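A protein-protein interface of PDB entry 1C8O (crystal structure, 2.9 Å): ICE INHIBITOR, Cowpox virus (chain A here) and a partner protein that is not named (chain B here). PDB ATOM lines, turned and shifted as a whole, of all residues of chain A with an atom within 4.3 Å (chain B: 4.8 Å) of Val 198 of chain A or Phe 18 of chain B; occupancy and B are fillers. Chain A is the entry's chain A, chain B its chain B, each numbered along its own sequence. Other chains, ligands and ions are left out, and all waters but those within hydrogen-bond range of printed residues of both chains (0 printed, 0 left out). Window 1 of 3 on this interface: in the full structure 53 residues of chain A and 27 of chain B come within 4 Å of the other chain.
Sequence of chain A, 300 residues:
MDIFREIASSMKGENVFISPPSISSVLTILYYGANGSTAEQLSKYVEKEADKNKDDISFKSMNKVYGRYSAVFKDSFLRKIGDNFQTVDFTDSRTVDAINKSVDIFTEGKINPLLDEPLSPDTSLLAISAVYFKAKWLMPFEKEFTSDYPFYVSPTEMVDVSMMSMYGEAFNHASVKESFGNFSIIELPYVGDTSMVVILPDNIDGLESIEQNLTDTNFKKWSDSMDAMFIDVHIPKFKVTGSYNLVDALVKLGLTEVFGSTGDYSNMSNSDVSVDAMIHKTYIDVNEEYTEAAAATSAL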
ATOM      1  N   SER A 184     -17.993  20.511  -3.672  1.00  0.00           N
ATOM      2  CA  SER A 184     -19.443  20.467  -3.668  1.00  0.00           C
ATOM      3  C   SER A 184     -19.839  21.608  -4.593  1.00  0.00           C
ATOM      4  O   SER A 184     -19.106  22.581  -4.717  1.00  0.00           O
ATOM      5  CB  SER A 184     -19.980  20.731  -2.264  1.00  0.00           C
ATOM      6  OG  SER A 184     -19.446  19.800  -1.342  1.00  0.00           O
ATOM      7  N   ILE A 185     -20.992  21.498  -5.235  1.00  0.00           N
ATOM      8  CA  ILE A 185     -21.422  22.530  -6.152  1.00  0.00           C
ATOM      9  C   ILE A 185     -22.909  22.724  -5.882  1.00  0.00           C
ATOM     10  O   ILE A 185     -23.645  21.761  -5.838  1.00  0.00           O
ATOM     11  CB  ILE A 185     -21.102  22.050  -7.591  1.00  0.00           C
ATOM     12  CG1 ILE A 185     -21.161  23.200  -8.576  1.00  0.00           C
ATOM     13  CG2 ILE A 185     -22.059  20.960  -8.004  1.00  0.00           C
ATOM     14  CD1 ILE A 185     -22.528  23.780  -8.761  1.00  0.00           C
ATOM     15  N   ILE A 186     -23.355  23.957  -5.676  1.00  0.00           N
ATOM     16  CA  ILE A 186     -24.759  24.189  -5.364  1.00  0.00           C
ATOM     17  C   ILE A 186     -25.330  25.324  -6.211  1.00  0.00           C
ATOM     18  O   ILE A 186     -24.576  26.118  -6.773  1.00  0.00           O
ATOM     19  CB  ILE A 186     -24.888  24.523  -3.875  1.00  0.00           C
ATOM     20  CG1 ILE A 186     -26.336  24.381  -3.419  1.00  0.00           C
ATOM     21  CG2 ILE A 186     -24.327  25.897  -3.622  1.00  0.00           C
ATOM     22  CD1 ILE A 186     -27.109  25.662  -3.261  1.00  0.00           C
ATOM     23  N   LEU A 188     -28.002  28.596  -6.172  1.00  0.00           N
ATOM     24  CA  LEU A 188     -28.880  29.525  -5.476  1.00  0.00           C
ATOM     25  C   LEU A 188     -29.573  30.304  -6.571  1.00  0.00           C
ATOM     26  O   LEU A 188     -29.003  31.188  -7.180  1.00  0.00           O
ATOM     27  CB  LEU A 188     -28.065  30.463  -4.597  1.00  0.00           C
ATOM     28  CG  LEU A 188     -27.267  29.771  -3.498  1.00  0.00           C
ATOM     29  CD1 LEU A 188     -25.841  30.286  -3.490  1.00  0.00           C
ATOM     30  CD2 LEU A 188     -27.953  30.017  -2.172  1.00  0.00           C
ATOM     31  N   MET A 196     -27.096  31.427  -9.268  1.00  0.00           N
ATOM     32  CA  MET A 196     -25.691  31.463  -8.903  1.00  0.00           C
ATOM     33  C   MET A 196     -25.261  30.056  -8.482  1.00  0.00           C
ATOM     34  O   MET A 196     -25.770  29.485  -7.515  1.00  0.00           O
ATOM     35  CB  MET A 196     -25.408  32.448  -7.763  1.00  0.00           C
ATOM     36  CG  MET A 196     -23.902  32.647  -7.556  1.00  0.00           C
ATOM     37  SD  MET A 196     -23.446  33.918  -6.383  1.00  0.00           S
ATOM     38  CE  MET A 196     -23.310  32.970  -4.889  1.00  0.00           C
ATOM     39  N   VAL A 197     -24.321  29.516  -9.244  1.00  0.00           N
ATOM     40  CA  VAL A 197     -23.776  28.198  -9.027  1.00  0.00           C
ATOM     41  C   VAL A 197     -22.418  28.346  -8.332  1.00  0.00           C
ATOM     42  O   VAL A 197     -21.447  28.761  -8.957  1.00  0.00           O
ATOM     43  CB  VAL A 197     -23.634  27.475 -10.398  1.00  0.00           C
ATOM     44  CG1 VAL A 197     -22.753  26.269 -10.282  1.00  0.00           C
ATOM     45  CG2 VAL A 197     -25.014  27.057 -10.905  1.00  0.00           C
ATOM     46  N   VAL A 198     -22.363  28.028  -7.035  1.00  0.00           N
ATOM     47  CA  VAL A 198     -21.120  28.119  -6.247  1.00  0.00           C
ATOM     48  C   VAL A 198     -20.371  26.783  -6.199  1.00  0.00           C
ATOM     49  O   VAL A 198     -20.970  25.744  -5.979  1.00  0.00           O
ATOM     50  CB  VAL A 198     -21.395  28.521  -4.788  1.00  0.00           C
ATOM     51  CG1 VAL A 198     -20.102  28.872  -4.107  1.00  0.00           C
ATOM     52  CG2 VAL A 198     -22.355  29.666  -4.737  1.00  0.00           C
ATOM     53  N   ILE A 199     -19.061  26.836  -6.399  1.00  0.00           N
ATOM     54  CA  ILE A 199     -18.194  25.667  -6.373  1.00  0.00           C
ATOM     55  C   ILE A 199     -17.303  25.817  -5.152  1.00  0.00           C
ATOM     56  O   ILE A 199     -16.412  26.660  -5.123  1.00  0.00           O
ATOM     57  CB  ILE A 199     -17.305  25.615  -7.636  1.00  0.00           C
ATOM     58  CG1 ILE A 199     -18.160  25.265  -8.845  1.00  0.00           C
ATOM     59  CG2 ILE A 199     -16.177  24.622  -7.462  1.00  0.00           C
ATOM     60  CD1 ILE A 199     -17.417  25.320 -10.160  1.00  0.00           C
ATOM     61  N   LEU A 200     -17.543  24.987  -4.145  1.00  0.00           N
ATOM     62  CA  LEU A 200     -16.787  25.034  -2.892  1.00  0.00           C
ATOM     63  C   LEU A 200     -15.901  23.793  -2.633  1.00  0.00           C
ATOM     64  O   LEU A 200     -16.408  22.737  -2.275  1.00  0.00           O
ATOM     65  CB  LEU A 200     -17.784  25.201  -1.751  1.00  0.00           C
ATOM     66  CG  LEU A 200     -17.171  25.202  -0.372  1.00  0.00           C
ATOM     67  CD1 LEU A 200     -16.151  26.306  -0.314  1.00  0.00           C
ATOM     68  CD2 LEU A 200     -18.247  25.383   0.680  1.00  0.00           C
ATOM     69  N   LEU A 207      -8.798  24.797  -3.727  1.00  0.00           N
ATOM     70  CA  LEU A 207      -9.364  25.616  -4.792  1.00  0.00           C
ATOM     71  C   LEU A 207      -8.501  25.717  -6.030  1.00  0.00           C
ATOM     72  O   LEU A 207      -9.014  25.646  -7.142  1.00  0.00           O
ATOM     73  CB  LEU A 207      -9.676  27.030  -4.289  1.00  0.00           C
ATOM     74  CG  LEU A 207     -10.372  27.971  -5.292  1.00  0.00           C
ATOM     75  CD1 LEU A 207     -11.615  27.303  -5.851  1.00  0.00           C
ATOM     76  CD2 LEU A 207     -10.739  29.283  -4.618  1.00  0.00           C
ATOM     77  N   PRO A 236     -21.058  33.811   2.285  1.00  0.00           N
ATOM     78  CA  PRO A 236     -20.715  35.172   2.707  1.00  0.00           C
ATOM     79  C   PRO A 236     -21.332  36.287   1.881  1.00  0.00           C
ATOM     80  O   PRO A 236     -21.292  36.250   0.646  1.00  0.00           O
ATOM     81  CB  PRO A 236     -19.197  35.181   2.604  1.00  0.00           C
ATOM     82  CG  PRO A 236     -18.988  34.394   1.365  1.00  0.00           C
ATOM     83  CD  PRO A 236     -19.929  33.205   1.557  1.00  0.00           C
ATOM     84  N   PHE B  12     -23.399  23.170   3.289  1.00  0.00           N
ATOM     85  CA  PHE B  12     -22.510  23.858   2.354  1.00  0.00           C
ATOM     86  C   PHE B  12     -22.063  25.175   3.003  1.00  0.00           C
ATOM     87  O   PHE B  12     -22.800  26.163   2.968  1.00  0.00           O
ATOM     88  CB  PHE B  12     -23.277  24.125   1.053  1.00  0.00           C
ATOM     89  CG  PHE B  12     -22.443  24.715  -0.058  1.00  0.00           C
ATOM     90  CD1 PHE B  12     -22.063  26.053  -0.036  1.00  0.00           C
ATOM     91  CD2 PHE B  12     -22.057  23.934  -1.142  1.00  0.00           C
ATOM     92  CE1 PHE B  12     -21.314  26.600  -1.074  1.00  0.00           C
ATOM     93  CE2 PHE B  12     -21.310  24.474  -2.183  1.00  0.00           C
ATOM     94  CZ  PHE B  12     -20.937  25.809  -2.148  1.00  0.00           C
ATOM     95  N   ALA B  14     -19.484  28.180   2.874  1.00  0.00           N
ATOM     96  CA  ALA B  14     -18.502  28.873   2.049  1.00  0.00           C
ATOM     97  C   ALA B  14     -17.565  29.758   2.858  1.00  0.00           C
ATOM     98  O   ALA B  14     -17.470  30.955   2.609  1.00  0.00           O
ATOM     99  CB  ALA B  14     -19.213  29.696   0.976  1.00  0.00           C
ATOM    100  N   HIS B  16     -14.230  29.636   2.940  1.00  0.00           N
ATOM    101  CA  HIS B  16     -12.882  29.538   2.397  1.00  0.00           C
ATOM    102  C   HIS B  16     -12.988  29.740   0.886  1.00  0.00           C
ATOM    103  O   HIS B  16     -14.075  29.633   0.323  1.00  0.00           O
ATOM    104  CB  HIS B  16     -12.169  28.221   2.798  1.00  0.00           C
ATOM    105  CG  HIS B  16     -12.841  26.961   2.340  1.00  0.00           C
ATOM    106  ND1 HIS B  16     -14.065  26.544   2.822  1.00  0.00           N
ATOM    107  CD2 HIS B  16     -12.432  26.000   1.478  1.00  0.00           C
ATOM    108  CE1 HIS B  16     -14.379  25.383   2.276  1.00  0.00           C
ATOM    109  NE2 HIS B  16     -13.404  25.030   1.459  1.00  0.00           N
ATOM    110  N   PRO B  17     -11.870  30.074   0.219  1.00  0.00           N
ATOM    111  CA  PRO B  17     -11.831  30.316  -1.226  1.00  0.00           C
ATOM    112  C   PRO B  17     -12.812  29.472  -2.018  1.00  0.00           C
ATOM    113  O   PRO B  17     -12.921  28.271  -1.789  1.00  0.00           O
ATOM    114  CB  PRO B  17     -10.390  30.014  -1.585  1.00  0.00           C
ATOM    115  CG  PRO B  17      -9.672  30.449  -0.379  1.00  0.00           C
ATOM    116  CD  PRO B  17     -10.506  29.903   0.740  1.00  0.00           C
ATOM    117  N   PHE B  18     -13.525  30.103  -2.945  1.00  0.00           N
ATOM    118  CA  PHE B  18     -14.496  29.400  -3.759  1.00  0.00           C
ATOM    119  C   PHE B  18     -14.794  30.107  -5.085  1.00  0.00           C
ATOM    120  O   PHE B  18     -14.451  31.272  -5.265  1.00  0.00           O
ATOM    121  CB  PHE B  18     -15.789  29.193  -2.960  1.00  0.00           C
ATOM    122  CG  PHE B  18     -16.546  30.461  -2.650  1.00  0.00           C
ATOM    123  CD1 PHE B  18     -17.355  31.054  -3.604  1.00  0.00           C
ATOM    124  CD2 PHE B  18     -16.490  31.025  -1.380  1.00  0.00           C
ATOM    125  CE1 PHE B  18     -18.098  32.184  -3.296  1.00  0.00           C
ATOM    126  CE2 PHE B  18     -17.230  32.153  -1.068  1.00  0.00           C
ATOM    127  CZ  PHE B  18     -18.034  32.730  -2.027  1.00  0.00           C
ATOM    128  N   ILE B  19     -15.415  29.380  -6.012  1.00  0.00           N
ATOM    129  CA  ILE B  19     -15.772  29.919  -7.310  1.00  0.00           C
ATOM    130  C   ILE B  19     -17.276  30.091  -7.378  1.00  0.00           C
ATOM    131  O   ILE B  19     -18.015  29.226  -6.937  1.00  0.00           O
ATOM    132  CB  ILE B  19     -15.387  28.971  -8.438  1.00  0.00           C
ATOM    133  CG1 ILE B  19     -13.919  28.566  -8.330  1.00  0.00           C
ATOM    134  CG2 ILE B  19     -15.680  29.633  -9.766  1.00  0.00           C
ATOM    135  CD1 ILE B  19     -12.915  29.672  -8.591  1.00  0.00           C
ATOM    136  N   TYR B  20     -17.735  31.210  -7.916  1.00  0.00           N
ATOM    137  CA  TYR B  20     -19.168  31.429  -8.059  1.00  0.00           C
ATOM    138  C   TYR B  20     -19.426  31.846  -9.491  1.00  0.00           C
ATOM    139  O   TYR B  20     -18.577  32.471 -10.118  1.00  0.00           O
ATOM    140  CB  TYR B  20     -19.704  32.492  -7.079  1.00  0.00           C
ATOM    141  CG  TYR B  20     -19.068  33.872  -7.144  1.00  0.00           C
ATOM    142  CD1 TYR B  20     -19.824  35.004  -7.457  1.00  0.00           C
ATOM    143  CD2 TYR B  20     -17.731  34.052  -6.826  1.00  0.00           C
ATOM    144  CE1 TYR B  20     -19.255  36.284  -7.444  1.00  0.00           C
ATOM    145  CE2 TYR B  20     -17.159  35.314  -6.811  1.00  0.00           C
ATOM    146  CZ  TYR B  20     -17.920  36.430  -7.119  1.00  0.00           C
ATOM    147  OH  TYR B  20     -17.318  37.675  -7.096  1.00  0.00           O
ATOM    148  N   GLY B  33     -16.446  34.549 -10.917  1.00  0.00           N
ATOM    149  CA  GLY B  33     -15.362  35.073 -10.118  1.00  0.00           C
ATOM    150  C   GLY B  33     -14.843  34.105  -9.072  1.00  0.00           C
ATOM    151  O   GLY B  33     -15.273  32.956  -9.000  1.00  0.00           O
ATOM    152  N   ARG B  34     -13.897  34.583  -8.269  1.00  0.00           N
ATOM    153  CA  ARG B  34     -13.292  33.804  -7.208  1.00  0.00           C
ATOM    154  C   ARG B  34     -13.314  34.627  -5.921  1.00  0.00           C
ATOM    155  O   ARG B  34     -12.914  35.779  -5.915  1.00  0.00           O
ATOM    156  CB  ARG B  34     -11.851  33.455  -7.562  1.00  0.00           C
ATOM    157  CG  ARG B  34     -11.189  32.552  -6.536  1.00  0.00           C
ATOM    158  CD  ARG B  34      -9.730  32.904  -6.348  1.00  0.00           C
ATOM    159  NE  ARG B  34      -8.952  32.718  -7.562  1.00  0.00           N
ATOM    160  CZ  ARG B  34      -7.803  33.339  -7.794  1.00  0.00           C
ATOM    161  NH1 ARG B  34      -7.319  34.178  -6.894  1.00  0.00           N
ATOM    162  NH2 ARG B  34      -7.142  33.133  -8.923  1.00  0.00           N
ATOM    163  N   TYR B  35     -13.783  34.034  -4.833  1.00  0.00           N
ATOM    164  CA  TYR B  35     -13.843  34.743  -3.569  1.00  0.00           C
ATOM    165  C   TYR B  35     -12.670  34.319  -2.691  1.00  0.00           C
ATOM    166  O   TYR B  35     -12.731  33.277  -2.042  1.00  0.00           O
ATOM    167  CB  TYR B  35     -15.147  34.416  -2.855  1.00  0.00           C
ATOM    168  CG  TYR B  35     -15.376  35.265  -1.641  1.00  0.00           C
ATOM    169  CD1 TYR B  35     -15.829  36.569  -1.762  1.00  0.00           C
ATOM    170  CD2 TYR B  35     -15.107  34.783  -0.369  1.00  0.00           C
ATOM    171  CE1 TYR B  35     -16.009  37.377  -0.650  1.00  0.00           C
ATOM    172  CE2 TYR B  35     -15.283  35.587   0.751  1.00  0.00           C
ATOM    173  CZ  TYR B  35     -15.736  36.884   0.601  1.00  0.00           C
ATOM    174  OH  TYR B  35     -15.910  37.688   1.702  1.00  0.00           O
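The backbone NH (N) of Ile 199 of chain A lies within hydrogen-bond range of the backbone carbonyl oxygen (O) of Ile 19 of chain B, 2.7 Å away.
The backbone carbonyl oxygen (O) of Ser 184 of chain A sits at hydrogen-bond distance from the backbone NH (N) of Leu 200 of chain A (2.9 Å).
The backbone NH (N) of Val 198 of chain A sits at hydrogen-bond distance from the backbone carbonyl oxygen (O) of Ile 186 of chain A (2.9 Å).
N of Leu 188 of chain A is in hydrogen-bond range of O of Met 196 of chain A (2.8 Å).
The backbone carbonyl oxygen of Phe 18 of chain B lies within hydrogen-bond range of the backbone NH of Tyr 35 of chain B (2.9 Å).
N of Gly 33 of chain B sits at hydrogen-bond distance from O of Tyr 20 of chain B.
Among the printed residues, merely in contact across the chains: Ser 184 of chain A with Phe 12 of chain B (3.9 Å), Ile 186 of chain A with Phe 12 of chain B (3.6 Å), Met 196 of chain A with Tyr 20 of chain B (3.9 Å), Val 197 of chain A with Tyr 20 of chain B (3.6 Å), Val 198 of chain A with Phe 12 of chain B (3.7 Å), Val 198 of chain A with Phe 18 of chain B (3.5 Å), Val 198 of chain A with Ile 19 of chain B (3.4 Å), Ile 199 of chain A with Phe 18 of chain B (3.4 Å), Leu 200 of chain A with Phe 12 of chain B (3.2 Å), Leu 200 of chain A with Ala 14 of chain B (3.8 Å), Leu 200 of chain A with His 16 of chain B (3.3 Å), Leu 200 of chain A with Phe 18 of chain B (3.9 Å), Leu 207 of chain A with Pro 17 of chain B (3.1 Å), Leu 207 of chain A with Phe 18 of chain B (3.4 Å), Leu 207 of chain A with Ile 19 of chain B (3.6 Å), Leu 207 of chain A with Arg 34 of chain B (3.8 Å), Pro 236 of chain A with Ala 14 of chain B (3.5 Å), Pro 236 of chain A with Phe 18 of chain B (3.7 Å) and Pro 236 of chain A with Tyr 35 of chain B (3.9 Å).
Phe 18 of chain B touches just these residues of chain A: Val 198 (3.5 Å), Ile 199 (3.4 Å), Leu 200 (3.9 Å), Leu 207 (3.4 Å) and Pro 236 (3.7 Å).
Printed residues of chain B within 4 Å of Ile 186 of chain A: Phe 12.
Printed residues of chain A within 4 Å of Tyr 20 of chain B: Met 196 and Val 197.
Of the printed residues of chain A, Ala 14 of chain B touches Leu 200 (3.8 Å) and Pro 236 (3.5 Å).
Of the printed residues of chain A, His 16 of chain B touches Leu 200 (3.3 Å).
The nearest residue of chain B that does not touch Val 198 of chain A is Tyr 20 of chain B (4.2 Å).
The nearest printed residue of chain A that does not touch Phe 18 of chain B is Met 196 of chain A (5.5 Å).
The nearest printed residue of chain A that does not touch Ala 14 of chain B is Val 198 of chain A (5.2 Å).
Printed residues of chain A that touch a printed residue of chain B: Ser 184, Ile 186, Met 196, Val 197, Val 198, Ile 199, Leu 200, Leu 207 and Pro 236.
Of the 10 printed residues of chain B, 9 touch a printed residue of chain A.
Hydrophobic or aromatic side chains of chain B that line the printed part of chain A: Phe 12, Ala 14, His 16, Pro 17, Phe 18, Ile 19, Tyr 20 and Tyr 35.
Among the printed residues, no Asp or Glu carboxylate lies within 4 Å of a Lys or Arg side-chain nitrogen of the other chain.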
